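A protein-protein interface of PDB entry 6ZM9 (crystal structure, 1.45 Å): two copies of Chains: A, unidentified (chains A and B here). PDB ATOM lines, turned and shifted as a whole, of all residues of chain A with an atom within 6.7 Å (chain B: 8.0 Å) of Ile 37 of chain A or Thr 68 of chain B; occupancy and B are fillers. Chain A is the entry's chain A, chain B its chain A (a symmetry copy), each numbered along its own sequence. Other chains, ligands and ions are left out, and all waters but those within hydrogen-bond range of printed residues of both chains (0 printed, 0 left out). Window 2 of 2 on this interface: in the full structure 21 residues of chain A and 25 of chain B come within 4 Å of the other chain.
O of Arg 55 of chain B lies within hydrogen-bond range of N of Phe 51 of chain A (2.8 Å).
The side-chain carboxylate of Glu 30 of chain A is in salt-bridge range of the guanidinium group of Arg 55 of chain B, at 2.9 Å.
The backbone carbonyl oxygen of Ser 71 of chain B is in hydrogen-bond range of the backbone NH of Gln 54 of chain B.
NH1 of Arg 55 of chain B lies within hydrogen-bond range of OD1 of Asn 70 of chain B (2.9 Å).
O of Pro 47 of chain A sits at hydrogen-bond distance from NH1 of Arg 40 of chain A (3.1 Å).
Among the printed residues, pairs that only touch across the chains: Phe 51 of chain A with Gln 54 of chain B, Pro 47 of chain A with Leu 66 of chain B, Ile 37 of chain A with Leu 66 of chain B, Glu 30 of chain A with Thr 68 of chain B, Phe 51 of chain A with Val 57 of chain B, Lys 41 of chain A with Leu 66 of chain B, Ile 37 of chain A with Thr 68 of chain B, Ile 37 of chain A with Val 57 of chain B, Val 33 of chain A with Thr 68 of chain B and Val 33 of chain A with Val 57 of chain B.
Of the printed residues of chain B, Glu 30 of chain A touches Arg 55 (2.9 Å) and Thr 68 (3.7 Å).
Of the printed residues of chain B, Val 33 of chain A touches Val 57 and Thr 68.
Ile 37 of chain A touches just these residues of chain B: Val 57 (3.8 Å), Leu 66 (3.7 Å) and Thr 68 (3.8 Å).
Of the printed residues of chain B, Lys 41 of chain A touches Leu 66.
Of the printed residues of chain A, Leu 66 of chain B touches Ile 37, Lys 41 and Pro 47.
The nearest printed residue of chain A that does not touch Thr 68 of chain B is Phe 51 of chain A (6.8 Å).
The nearest printed residue of chain A that does not touch Arg 55 of chain B is Val 33 of chain A (4.05 Å).
Of the 18 printed residues of chain B, 5 touch a printed residue of chain A.
Printed residues of chain A that touch a printed residue of chain B: Glu 30, Val 33, Ile 37, Lys 41, Pro 47 and Phe 51.
Among the printed residues, Asp or Glu carboxylates within 4 Å of a Lys or Arg side-chain nitrogen of the other chain: Glu 30 of chain A with Arg 55 of chain B (2.9 Å).
No position is printed for both chains.
Of the 12 pairs that touch across the chains among the printed residues, none has its exchanged pair printed and touching as well.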
ATOM      1  N   GLU A  30       7.460   8.322 -17.636  1.00  0.00           N
ATOM      2  CA  GLU A  30       7.105   8.579 -16.239  1.00  0.00           C
ATOM      3  C   GLU A  30       6.204   9.797 -16.096  1.00  0.00           C
ATOM      4  O   GLU A  30       5.352   9.838 -15.195  1.00  0.00           O
ATOM      5  CB  GLU A  30       8.331   8.700 -15.341  1.00  0.00           C
ATOM      6  CG  GLU A  30       7.992   8.323 -13.878  1.00  0.00           C
ATOM      7  CD  GLU A  30       7.669   6.829 -13.630  1.00  0.00           C
ATOM      8  OE1 GLU A  30       7.805   5.976 -14.546  1.00  0.00           O
ATOM      9  OE2 GLU A  30       7.275   6.496 -12.488  1.00  0.00           O
ATOM     10  N   VAL A  32       3.818  10.562 -18.163  1.00  0.00           N
ATOM     11  CA  VAL A  32       2.486  10.045 -18.453  1.00  0.00           C
ATOM     12  C   VAL A  32       1.950   9.224 -17.287  1.00  0.00           C
ATOM     13  O   VAL A  32       0.766   9.324 -16.950  1.00  0.00           O
ATOM     14  CB  VAL A  32       2.499   9.258 -19.778  1.00  0.00           C
ATOM     15  CG1 VAL A  32       1.164   8.607 -20.028  1.00  0.00           C
ATOM     16  CG2 VAL A  32       2.873  10.181 -20.929  1.00  0.00           C
ATOM     17  N   VAL A  33       2.804   8.405 -16.658  1.00  0.00           N
ATOM     18  CA  VAL A  33       2.404   7.641 -15.471  1.00  0.00           C
ATOM     19  C   VAL A  33       1.865   8.578 -14.401  1.00  0.00           C
ATOM     20  O   VAL A  33       0.761   8.397 -13.875  1.00  0.00           O
ATOM     21  CB  VAL A  33       3.581   6.806 -14.937  1.00  0.00           C
ATOM     22  CG1 VAL A  33       3.215   6.124 -13.619  1.00  0.00           C
ATOM     23  CG2 VAL A  33       4.016   5.741 -15.958  1.00  0.00           C
ATOM     24  N   LYS A  34       2.662   9.584 -14.041  1.00  0.00           N
ATOM     25  CA  LYS A  34       2.272  10.480 -12.960  1.00  0.00           C
ATOM     26  C   LYS A  34       1.008  11.256 -13.307  1.00  0.00           C
ATOM     27  O   LYS A  34       0.137  11.450 -12.450  1.00  0.00           O
ATOM     28  CB  LYS A  34       3.428  11.428 -12.641  1.00  0.00           C
ATOM     29  CG  LYS A  34       4.661  10.785 -11.997  1.00  0.00           C
ATOM     30  CD  LYS A  34       5.765  11.828 -11.804  1.00  0.00           C
ATOM     31  CE  LYS A  34       7.037  11.216 -11.291  1.00  0.00           C
ATOM     32  NZ  LYS A  34       6.776  10.561  -9.992  1.00  0.00           N
ATOM     33  N   ASP A  35       0.905  11.754 -14.539  1.00  0.00           N
ATOM     34  CA  ASP A  35      -0.265  12.541 -14.919  1.00  0.00           C
ATOM     35  C   ASP A  35      -1.516  11.671 -14.924  1.00  0.00           C
ATOM     36  O   ASP A  35      -2.588  12.125 -14.494  1.00  0.00           O
ATOM     37  CB  ASP A  35      -0.036  13.211 -16.275  1.00  0.00           C
ATOM     38  CG  ASP A  35      -0.950  14.389 -16.518  1.00  0.00           C
ATOM     39  OD1 ASP A  35      -1.092  15.228 -15.612  1.00  0.00           O
ATOM     40  OD2 ASP A  35      -1.507  14.482 -17.630  1.00  0.00           O
ATOM     41  N   THR A  36      -1.398  10.424 -15.403  1.00  0.00           N
ATOM     42  CA  THR A  36      -2.536   9.512 -15.413  1.00  0.00           C
ATOM     43  C   THR A  36      -3.012   9.225 -13.993  1.00  0.00           C
ATOM     44  O   THR A  36      -4.222   9.212 -13.733  1.00  0.00           O
ATOM     45  CB  THR A  36      -2.170   8.220 -16.149  1.00  0.00           C
ATOM     46  OG1 THR A  36      -1.878   8.508 -17.523  1.00  0.00           O
ATOM     47  CG2 THR A  36      -3.307   7.215 -16.106  1.00  0.00           C
ATOM     48  N   ILE A  37      -2.085   8.976 -13.063  1.00  0.00           N
ATOM     49  CA  ILE A  37      -2.472   8.736 -11.673  1.00  0.00           C
ATOM     50  C   ILE A  37      -3.260   9.924 -11.139  1.00  0.00           C
ATOM     51  O   ILE A  37      -4.306   9.769 -10.497  1.00  0.00           O
ATOM     52  CB  ILE A  37      -1.236   8.458 -10.794  1.00  0.00           C
ATOM     53  CG1 ILE A  37      -0.600   7.113 -11.129  1.00  0.00           C
ATOM     54  CG2 ILE A  37      -1.621   8.541  -9.295  1.00  0.00           C
ATOM     55  CD1 ILE A  37       0.768   6.935 -10.510  1.00  0.00           C
ATOM     56  N   ALA A  38      -2.756  11.134 -11.393  1.00  0.00           N
ATOM     57  CA  ALA A  38      -3.398  12.338 -10.885  1.00  0.00           C
ATOM     58  C   ALA A  38      -4.794  12.522 -11.464  1.00  0.00           C
ATOM     59  O   ALA A  38      -5.730  12.861 -10.740  1.00  0.00           O
ATOM     60  CB  ALA A  38      -2.512  13.545 -11.204  1.00  0.00           C
ATOM     61  N   ILE A  39      -4.957  12.296 -12.763  1.00  0.00           N
ATOM     62  CA  ILE A  39      -6.257  12.462 -13.395  1.00  0.00           C
ATOM     63  C   ILE A  39      -7.244  11.438 -12.845  1.00  0.00           C
ATOM     64  O   ILE A  39      -8.392  11.765 -12.517  1.00  0.00           O
ATOM     65  CB  ILE A  39      -6.123  12.332 -14.921  1.00  0.00           C
ATOM     66  CG1 ILE A  39      -5.363  13.511 -15.515  1.00  0.00           C
ATOM     67  CG2 ILE A  39      -7.486  12.217 -15.556  1.00  0.00           C
ATOM     68  CD1 ILE A  39      -4.810  13.262 -16.901  1.00  0.00           C
ATOM     69  N   ARG A  40      -6.818  10.179 -12.753  1.00  0.00           N
ATOM     70  CA  ARG A  40      -7.716   9.117 -12.318  1.00  0.00           C
ATOM     71  C   ARG A  40      -8.099   9.282 -10.853  1.00  0.00           C
ATOM     72  O   ARG A  40      -9.243   9.005 -10.476  1.00  0.00           O
ATOM     73  CB  ARG A  40      -7.111   7.743 -12.632  1.00  0.00           C
ATOM     74  CG  ARG A  40      -6.867   7.567 -14.141  1.00  0.00           C
ATOM     75  CD  ARG A  40      -6.576   6.145 -14.532  1.00  0.00           C
ATOM     76  NE  ARG A  40      -7.821   5.413 -14.719  1.00  0.00           N
ATOM     77  CZ  ARG A  40      -7.929   4.095 -14.663  1.00  0.00           C
ATOM     78  NH1 ARG A  40      -6.859   3.351 -14.415  1.00  0.00           N
ATOM     79  NH2 ARG A  40      -9.102   3.512 -14.859  1.00  0.00           N
ATOM     80  N   LYS A  41      -7.185   9.767 -10.017  1.00  0.00           N
ATOM     81  CA  LYS A  41      -7.563  10.056  -8.637  1.00  0.00           C
ATOM     82  C   LYS A  41      -8.664  11.112  -8.576  1.00  0.00           C
ATOM     83  O   LYS A  41      -9.600  10.995  -7.772  1.00  0.00           O
ATOM     84  CB  LYS A  41      -6.341  10.486  -7.841  1.00  0.00           C
ATOM     85  CG  LYS A  41      -5.389   9.355  -7.478  1.00  0.00           C
ATOM     86  CD  LYS A  41      -4.222   9.899  -6.662  1.00  0.00           C
ATOM     87  CE  LYS A  41      -3.334   8.814  -6.072  1.00  0.00           C
ATOM     88  NZ  LYS A  41      -2.070   9.409  -5.499  1.00  0.00           N
ATOM     89  N   ARG A  42      -8.586  12.147  -9.420  1.00  0.00           N
ATOM     90  CA  ARG A  42      -9.617  13.187  -9.417  1.00  0.00           C
ATOM     91  C   ARG A  42     -10.946  12.670  -9.950  1.00  0.00           C
ATOM     92  O   ARG A  42     -11.993  13.253  -9.648  1.00  0.00           O
ATOM     93  CB  ARG A  42      -9.144  14.402 -10.209  1.00  0.00           C
ATOM     94  CG  ARG A  42      -8.065  15.197  -9.490  1.00  0.00           C
ATOM     95  CD  ARG A  42      -7.810  16.543 -10.175  1.00  0.00           C
ATOM     96  NE  ARG A  42      -7.324  16.389 -11.545  1.00  0.00           N
ATOM     97  CZ  ARG A  42      -6.039  16.389 -11.905  1.00  0.00           C
ATOM     98  NH1 ARG A  42      -5.077  16.546 -10.999  1.00  0.00           N
ATOM     99  NH2 ARG A  42      -5.716  16.246 -13.183  1.00  0.00           N
ATOM    100  N   ILE A  45     -11.559   7.060  -9.256  1.00  0.00           N
ATOM    101  CA  ILE A  45     -11.431   5.685  -9.750  1.00  0.00           C
ATOM    102  C   ILE A  45     -10.085   5.119  -9.339  1.00  0.00           C
ATOM    103  O   ILE A  45      -9.120   5.858  -9.116  1.00  0.00           O
ATOM    104  CB  ILE A  45     -11.620   5.707 -11.285  1.00  0.00           C
ATOM    105  CG1 ILE A  45     -11.833   4.317 -11.897  1.00  0.00           C
ATOM    106  CG2 ILE A  45     -10.413   6.280 -11.982  1.00  0.00           C
ATOM    107  CD1 ILE A  45     -12.311   4.337 -13.364  1.00  0.00           C
ATOM    108  N   PRO A  47      -6.556   3.942  -9.869  1.00  0.00           N
ATOM    109  CA  PRO A  47      -5.688   4.333 -10.990  1.00  0.00           C
ATOM    110  C   PRO A  47      -4.954   3.182 -11.654  1.00  0.00           C
ATOM    111  O   PRO A  47      -4.313   3.408 -12.698  1.00  0.00           O
ATOM    112  CB  PRO A  47      -4.686   5.298 -10.348  1.00  0.00           C
ATOM    113  CG  PRO A  47      -4.690   4.996  -8.930  1.00  0.00           C
ATOM    114  CD  PRO A  47      -6.015   4.383  -8.572  1.00  0.00           C
ATOM    115  N   PHE A  51       1.694   0.692 -18.319  1.00  0.00           N
ATOM    116  CA  PHE A  51       2.209   1.706 -19.232  1.00  0.00           C
ATOM    117  C   PHE A  51       3.383   1.100 -19.995  1.00  0.00           C
ATOM    118  O   PHE A  51       4.376   0.693 -19.393  1.00  0.00           O
ATOM    119  CB  PHE A  51       2.669   2.935 -18.457  1.00  0.00           C
ATOM    120  CG  PHE A  51       1.581   3.591 -17.620  1.00  0.00           C
ATOM    121  CD1 PHE A  51       1.218   3.055 -16.402  1.00  0.00           C
ATOM    122  CD2 PHE A  51       0.926   4.723 -18.070  1.00  0.00           C
ATOM    123  CE1 PHE A  51       0.237   3.649 -15.638  1.00  0.00           C
ATOM    124  CE2 PHE A  51      -0.060   5.319 -17.310  1.00  0.00           C
ATOM    125  CZ  PHE A  51      -0.396   4.788 -16.087  1.00  0.00           C
ATOM    126  N   LEU A  94     -10.107  10.871 -19.568  1.00  0.00           N
ATOM    127  CA  LEU A  94      -8.675  10.702 -19.372  1.00  0.00           C
ATOM    128  C   LEU A  94      -7.908  10.987 -20.657  1.00  0.00           C
ATOM    129  O   LEU A  94      -6.912  11.716 -20.653  1.00  0.00           O
ATOM    130  CB  LEU A  94      -8.403   9.288 -18.860  1.00  0.00           C
ATOM    131  CG  LEU A  94      -6.938   8.835 -18.796  1.00  0.00           C
ATOM    132  CD1 LEU A  94      -6.092   9.688 -17.853  1.00  0.00           C
ATOM    133  CD2 LEU A  94      -6.888   7.368 -18.378  1.00  0.00           C
ATOM    134  N   ASN B  20       8.271  -5.173  -8.029  1.00  0.00           N
ATOM    135  CA  ASN B  20       8.468  -4.706  -6.672  1.00  0.00           C
ATOM    136  C   ASN B  20       7.976  -5.771  -5.703  1.00  0.00           C
ATOM    137  O   ASN B  20       7.043  -6.522  -6.007  1.00  0.00           O
ATOM    138  CB  ASN B  20       7.590  -3.485  -6.382  1.00  0.00           C
ATOM    139  CG  ASN B  20       8.298  -2.160  -6.578  1.00  0.00           C
ATOM    140  OD1 ASN B  20       9.176  -2.013  -7.427  1.00  0.00           O
ATOM    141  ND2 ASN B  20       7.860  -1.156  -5.821  1.00  0.00           N
ATOM    142  N   GLY B  22       6.257  -5.071  -2.323  1.00  0.00           N
ATOM    143  CA  GLY B  22       5.793  -3.876  -1.632  1.00  0.00           C
ATOM    144  C   GLY B  22       6.335  -2.635  -2.317  1.00  0.00           C
ATOM    145  O   GLY B  22       6.213  -2.475  -3.535  1.00  0.00           O
ATOM    146  N   ASP B  23       6.951  -1.741  -1.549  1.00  0.00           N
ATOM    147  CA  ASP B  23       7.486  -0.514  -2.129  1.00  0.00           C
ATOM    148  C   ASP B  23       8.935  -0.652  -2.610  1.00  0.00           C
ATOM    149  O   ASP B  23       9.519   0.352  -3.031  1.00  0.00           O
ATOM    150  CB  ASP B  23       7.338   0.670  -1.165  1.00  0.00           C
ATOM    151  CG  ASP B  23       8.117   0.491   0.120  1.00  0.00           C
ATOM    152  OD1 ASP B  23       9.033  -0.357   0.160  1.00  0.00           O
ATOM    153  OD2 ASP B  23       7.802   1.201   1.099  1.00  0.00           O
ATOM    154  N   LYS B  24       9.504  -1.870  -2.616  1.00  0.00           N
ATOM    155  CA  LYS B  24      10.921  -2.075  -2.935  1.00  0.00           C
ATOM    156  C   LYS B  24      11.137  -2.695  -4.306  1.00  0.00           C
ATOM    157  O   LYS B  24      10.784  -3.866  -4.520  1.00  0.00           O
ATOM    158  CB  LYS B  24      11.558  -2.976  -1.872  1.00  0.00           C
ATOM    159  CG  LYS B  24      13.047  -3.232  -2.066  1.00  0.00           C
ATOM    160  CD  LYS B  24      13.614  -4.033  -0.886  1.00  0.00           C
ATOM    161  CE  LYS B  24      15.111  -4.293  -1.035  1.00  0.00           C
ATOM    162  NZ  LYS B  24      15.401  -5.485  -1.885  1.00  0.00           N
ATOM    163  N   PRO B  25      11.766  -1.982  -5.236  1.00  0.00           N
ATOM    164  CA  PRO B  25      12.154  -2.615  -6.503  1.00  0.00           C
ATOM    165  C   PRO B  25      13.087  -3.790  -6.229  1.00  0.00           C
ATOM    166  O   PRO B  25      14.089  -3.658  -5.521  1.00  0.00           O
ATOM    167  CB  PRO B  25      12.844  -1.480  -7.269  1.00  0.00           C
ATOM    168  CG  PRO B  25      12.304  -0.224  -6.652  1.00  0.00           C
ATOM    169  CD  PRO B  25      12.129  -0.557  -5.199  1.00  0.00           C
ATOM    170  N   GLN B  54       7.245  -2.911 -18.613  1.00  0.00           N
ATOM    171  CA  GLN B  54       6.225  -1.907 -18.394  1.00  0.00           C
ATOM    172  C   GLN B  54       6.539  -1.134 -17.128  1.00  0.00           C
ATOM    173  O   GLN B  54       7.319  -1.577 -16.279  1.00  0.00           O
ATOM    174  CB  GLN B  54       4.843  -2.514 -18.117  1.00  0.00           C
ATOM    175  CG  GLN B  54       4.450  -3.595 -19.047  1.00  0.00           C
ATOM    176  CD  GLN B  54       3.028  -4.049 -18.835  1.00  0.00           C
ATOM    177  OE1 GLN B  54       2.237  -4.088 -19.770  1.00  0.00           O
ATOM    178  NE2 GLN B  54       2.709  -4.448 -17.611  1.00  0.00           N
ATOM    179  N   ARG B  55       5.892   0.017 -16.997  1.00  0.00           N
ATOM    180  CA  ARG B  55       5.667   0.642 -15.699  1.00  0.00           C
ATOM    181  C   ARG B  55       4.245   0.290 -15.289  1.00  0.00           C
ATOM    182  O   ARG B  55       3.327   0.307 -16.115  1.00  0.00           O
ATOM    183  CB  ARG B  55       5.867   2.150 -15.738  1.00  0.00           C
ATOM    184  CG  ARG B  55       7.297   2.533 -16.043  1.00  0.00           C
ATOM    185  CD  ARG B  55       8.254   2.225 -14.895  1.00  0.00           C
ATOM    186  NE  ARG B  55       8.124   3.188 -13.812  1.00  0.00           N
ATOM    187  CZ  ARG B  55       8.598   3.012 -12.584  1.00  0.00           C
ATOM    188  NH1 ARG B  55       9.219   1.893 -12.243  1.00  0.00           N
ATOM    189  NH2 ARG B  55       8.443   3.978 -11.689  1.00  0.00           N
ATOM    190  N   GLY B  56       4.067  -0.077 -14.029  1.00  0.00           N
ATOM    191  CA  GLY B  56       2.768  -0.483 -13.540  1.00  0.00           C
ATOM    192  C   GLY B  56       2.392   0.294 -12.299  1.00  0.00           C
ATOM    193  O   GLY B  56       3.238   0.701 -11.504  1.00  0.00           O
ATOM    194  N   VAL B  57       1.084   0.470 -12.132  1.00  0.00           N
ATOM    195  CA  VAL B  57       0.499   1.119 -10.967  1.00  0.00           C
ATOM    196  C   VAL B  57      -0.503   0.143 -10.372  1.00  0.00           C
ATOM    197  O   VAL B  57      -1.361  -0.387 -11.093  1.00  0.00           O
ATOM    198  CB  VAL B  57      -0.183   2.439 -11.362  1.00  0.00           C
ATOM    199  CG1 VAL B  57      -0.914   3.064 -10.200  1.00  0.00           C
ATOM    200  CG2 VAL B  57       0.844   3.405 -11.937  1.00  0.00           C
ATOM    201  N   TYR B  58      -0.389  -0.096  -9.065  1.00  0.00           N
ATOM    202  CA  TYR B  58      -1.217  -1.048  -8.346  1.00  0.00           C
ATOM    203  C   TYR B  58      -1.553  -0.524  -6.960  1.00  0.00           C
ATOM    204  O   TYR B  58      -0.686  -0.012  -6.254  1.00  0.00           O
ATOM    205  CB  TYR B  58      -0.464  -2.354  -8.202  1.00  0.00           C
ATOM    206  CG  TYR B  58      -1.121  -3.421  -7.357  1.00  0.00           C
ATOM    207  CD1 TYR B  58      -2.150  -4.194  -7.871  1.00  0.00           C
ATOM    208  CD2 TYR B  58      -0.709  -3.659  -6.063  1.00  0.00           C
ATOM    209  CE1 TYR B  58      -2.747  -5.204  -7.115  1.00  0.00           C
ATOM    210  CE2 TYR B  58      -1.288  -4.672  -5.303  1.00  0.00           C
ATOM    211  CZ  TYR B  58      -2.322  -5.429  -5.833  1.00  0.00           C
ATOM    212  OH  TYR B  58      -2.915  -6.439  -5.095  1.00  0.00           O
ATOM    213  N   THR B  59      -2.810  -0.694  -6.557  1.00  0.00           N
ATOM    214  CA  THR B  59      -3.244  -0.339  -5.216  1.00  0.00           C
ATOM    215  C   THR B  59      -3.202  -1.586  -4.347  1.00  0.00           C
ATOM    216  O   THR B  59      -3.926  -2.553  -4.610  1.00  0.00           O
ATOM    217  CB  THR B  59      -4.655   0.241  -5.231  1.00  0.00           C
ATOM    218  OG1 THR B  59      -4.681   1.406  -6.056  1.00  0.00           O
ATOM    219  CG2 THR B  59      -5.079   0.624  -3.809  1.00  0.00           C
ATOM    220  N   GLN B  65      -2.133   1.385  -0.118  1.00  0.00           N
ATOM    221  CA  GLN B  65      -0.999   2.125  -0.650  1.00  0.00           C
ATOM    222  C   GLN B  65      -0.888   1.942  -2.159  1.00  0.00           C
ATOM    223  O   GLN B  65      -1.005   0.828  -2.677  1.00  0.00           O
ATOM    224  CB  GLN B  65       0.267   1.599   0.035  1.00  0.00           C
ATOM    225  CG  GLN B  65       1.565   2.311  -0.353  1.00  0.00           C
ATOM    226  CD  GLN B  65       2.812   1.684   0.280  1.00  0.00           C
ATOM    227  OE1 GLN B  65       2.719   0.976   1.287  1.00  0.00           O
ATOM    228  NE2 GLN B  65       3.980   1.950  -0.305  1.00  0.00           N
ATOM    229  N   LEU B  66      -0.625   3.036  -2.866  1.00  0.00           N
ATOM    230  CA  LEU B  66      -0.441   2.992  -4.311  1.00  0.00           C
ATOM    231  C   LEU B  66       1.034   2.782  -4.613  1.00  0.00           C
ATOM    232  O   LEU B  66       1.880   3.575  -4.191  1.00  0.00           O
ATOM    233  CB  LEU B  66      -0.909   4.313  -4.914  1.00  0.00           C
ATOM    234  CG  LEU B  66      -1.039   4.316  -6.435  1.00  0.00           C
ATOM    235  CD1 LEU B  66      -2.132   3.358  -6.842  1.00  0.00           C
ATOM    236  CD2 LEU B  66      -1.343   5.708  -6.941  1.00  0.00           C
ATOM    237  N   VAL B  67       1.341   1.733  -5.371  1.00  0.00           N
ATOM    238  CA  VAL B  67       2.704   1.414  -5.773  1.00  0.00           C
ATOM    239  C   VAL B  67       2.867   1.663  -7.264  1.00  0.00           C
ATOM    240  O   VAL B  67       2.015   1.269  -8.065  1.00  0.00           O
ATOM    241  CB  VAL B  67       2.994  -0.064  -5.444  1.00  0.00           C
ATOM    242  CG1 VAL B  67       4.383  -0.469  -5.927  1.00  0.00           C
ATOM    243  CG2 VAL B  67       2.845  -0.324  -3.962  1.00  0.00           C
ATOM    244  N   THR B  68       3.982   2.297  -7.634  1.00  0.00           N
ATOM    245  CA  THR B  68       4.446   2.402  -9.011  1.00  0.00           C
ATOM    246  C   THR B  68       5.723   1.570  -9.127  1.00  0.00           C
ATOM    247  O   THR B  68       6.672   1.768  -8.355  1.00  0.00           O
ATOM    248  CB  THR B  68       4.686   3.864  -9.400  1.00  0.00           C
ATOM    249  OG1 THR B  68       3.490   4.636  -9.201  1.00  0.00           O
ATOM    250  CG2 THR B  68       5.046   3.981 -10.865  1.00  0.00           C
ATOM    251  N   GLU B  69       5.755   0.657 -10.096  1.00  0.00           N
ATOM    252  CA  GLU B  69       6.816  -0.332 -10.169  1.00  0.00           C
ATOM    253  C   GLU B  69       7.144  -0.621 -11.629  1.00  0.00           C
ATOM    254  O   GLU B  69       6.406  -0.257 -12.544  1.00  0.00           O
ATOM    255  CB  GLU B  69       6.386  -1.652  -9.493  1.00  0.00           C
ATOM    256  CG  GLU B  69       5.127  -2.268 -10.120  1.00  0.00           C
ATOM    257  CD  GLU B  69       4.687  -3.585  -9.482  1.00  0.00           C
ATOM    258  OE1 GLU B  69       5.384  -4.117  -8.588  1.00  0.00           O
ATOM    259  OE2 GLU B  69       3.624  -4.097  -9.891  1.00  0.00           O
ATOM    260  N   ASN B  70       8.263  -1.300 -11.838  1.00  0.00           N
ATOM    261  CA  ASN B  70       8.459  -2.001 -13.094  1.00  0.00           C
ATOM    262  C   ASN B  70       7.633  -3.283 -13.066  1.00  0.00           C
ATOM    263  O   ASN B  70       7.449  -3.892 -12.014  1.00  0.00           O
ATOM    264  CB  ASN B  70       9.923  -2.375 -13.280  1.00  0.00           C
ATOM    265  CG  ASN B  70      10.817  -1.177 -13.456  1.00  0.00           C
ATOM    266  OD1 ASN B  70      10.402  -0.116 -13.928  1.00  0.00           O
ATOM    267  ND2 ASN B  70      12.080  -1.353 -13.107  1.00  0.00           N
ATOM    268  N   SER B  71       7.118  -3.681 -14.225  1.00  0.00           N
ATOM    269  CA  SER B  71       6.362  -4.915 -14.320  1.00  0.00           C
ATOM    270  C   SER B  71       6.585  -5.536 -15.693  1.00  0.00           C
ATOM    271  O   SER B  71       7.264  -4.974 -16.556  1.00  0.00           O
ATOM    272  CB  SER B  71       4.874  -4.707 -14.034  1.00  0.00           C
ATOM    273  OG  SER B  71       4.290  -3.867 -15.006  1.00  0.00           O
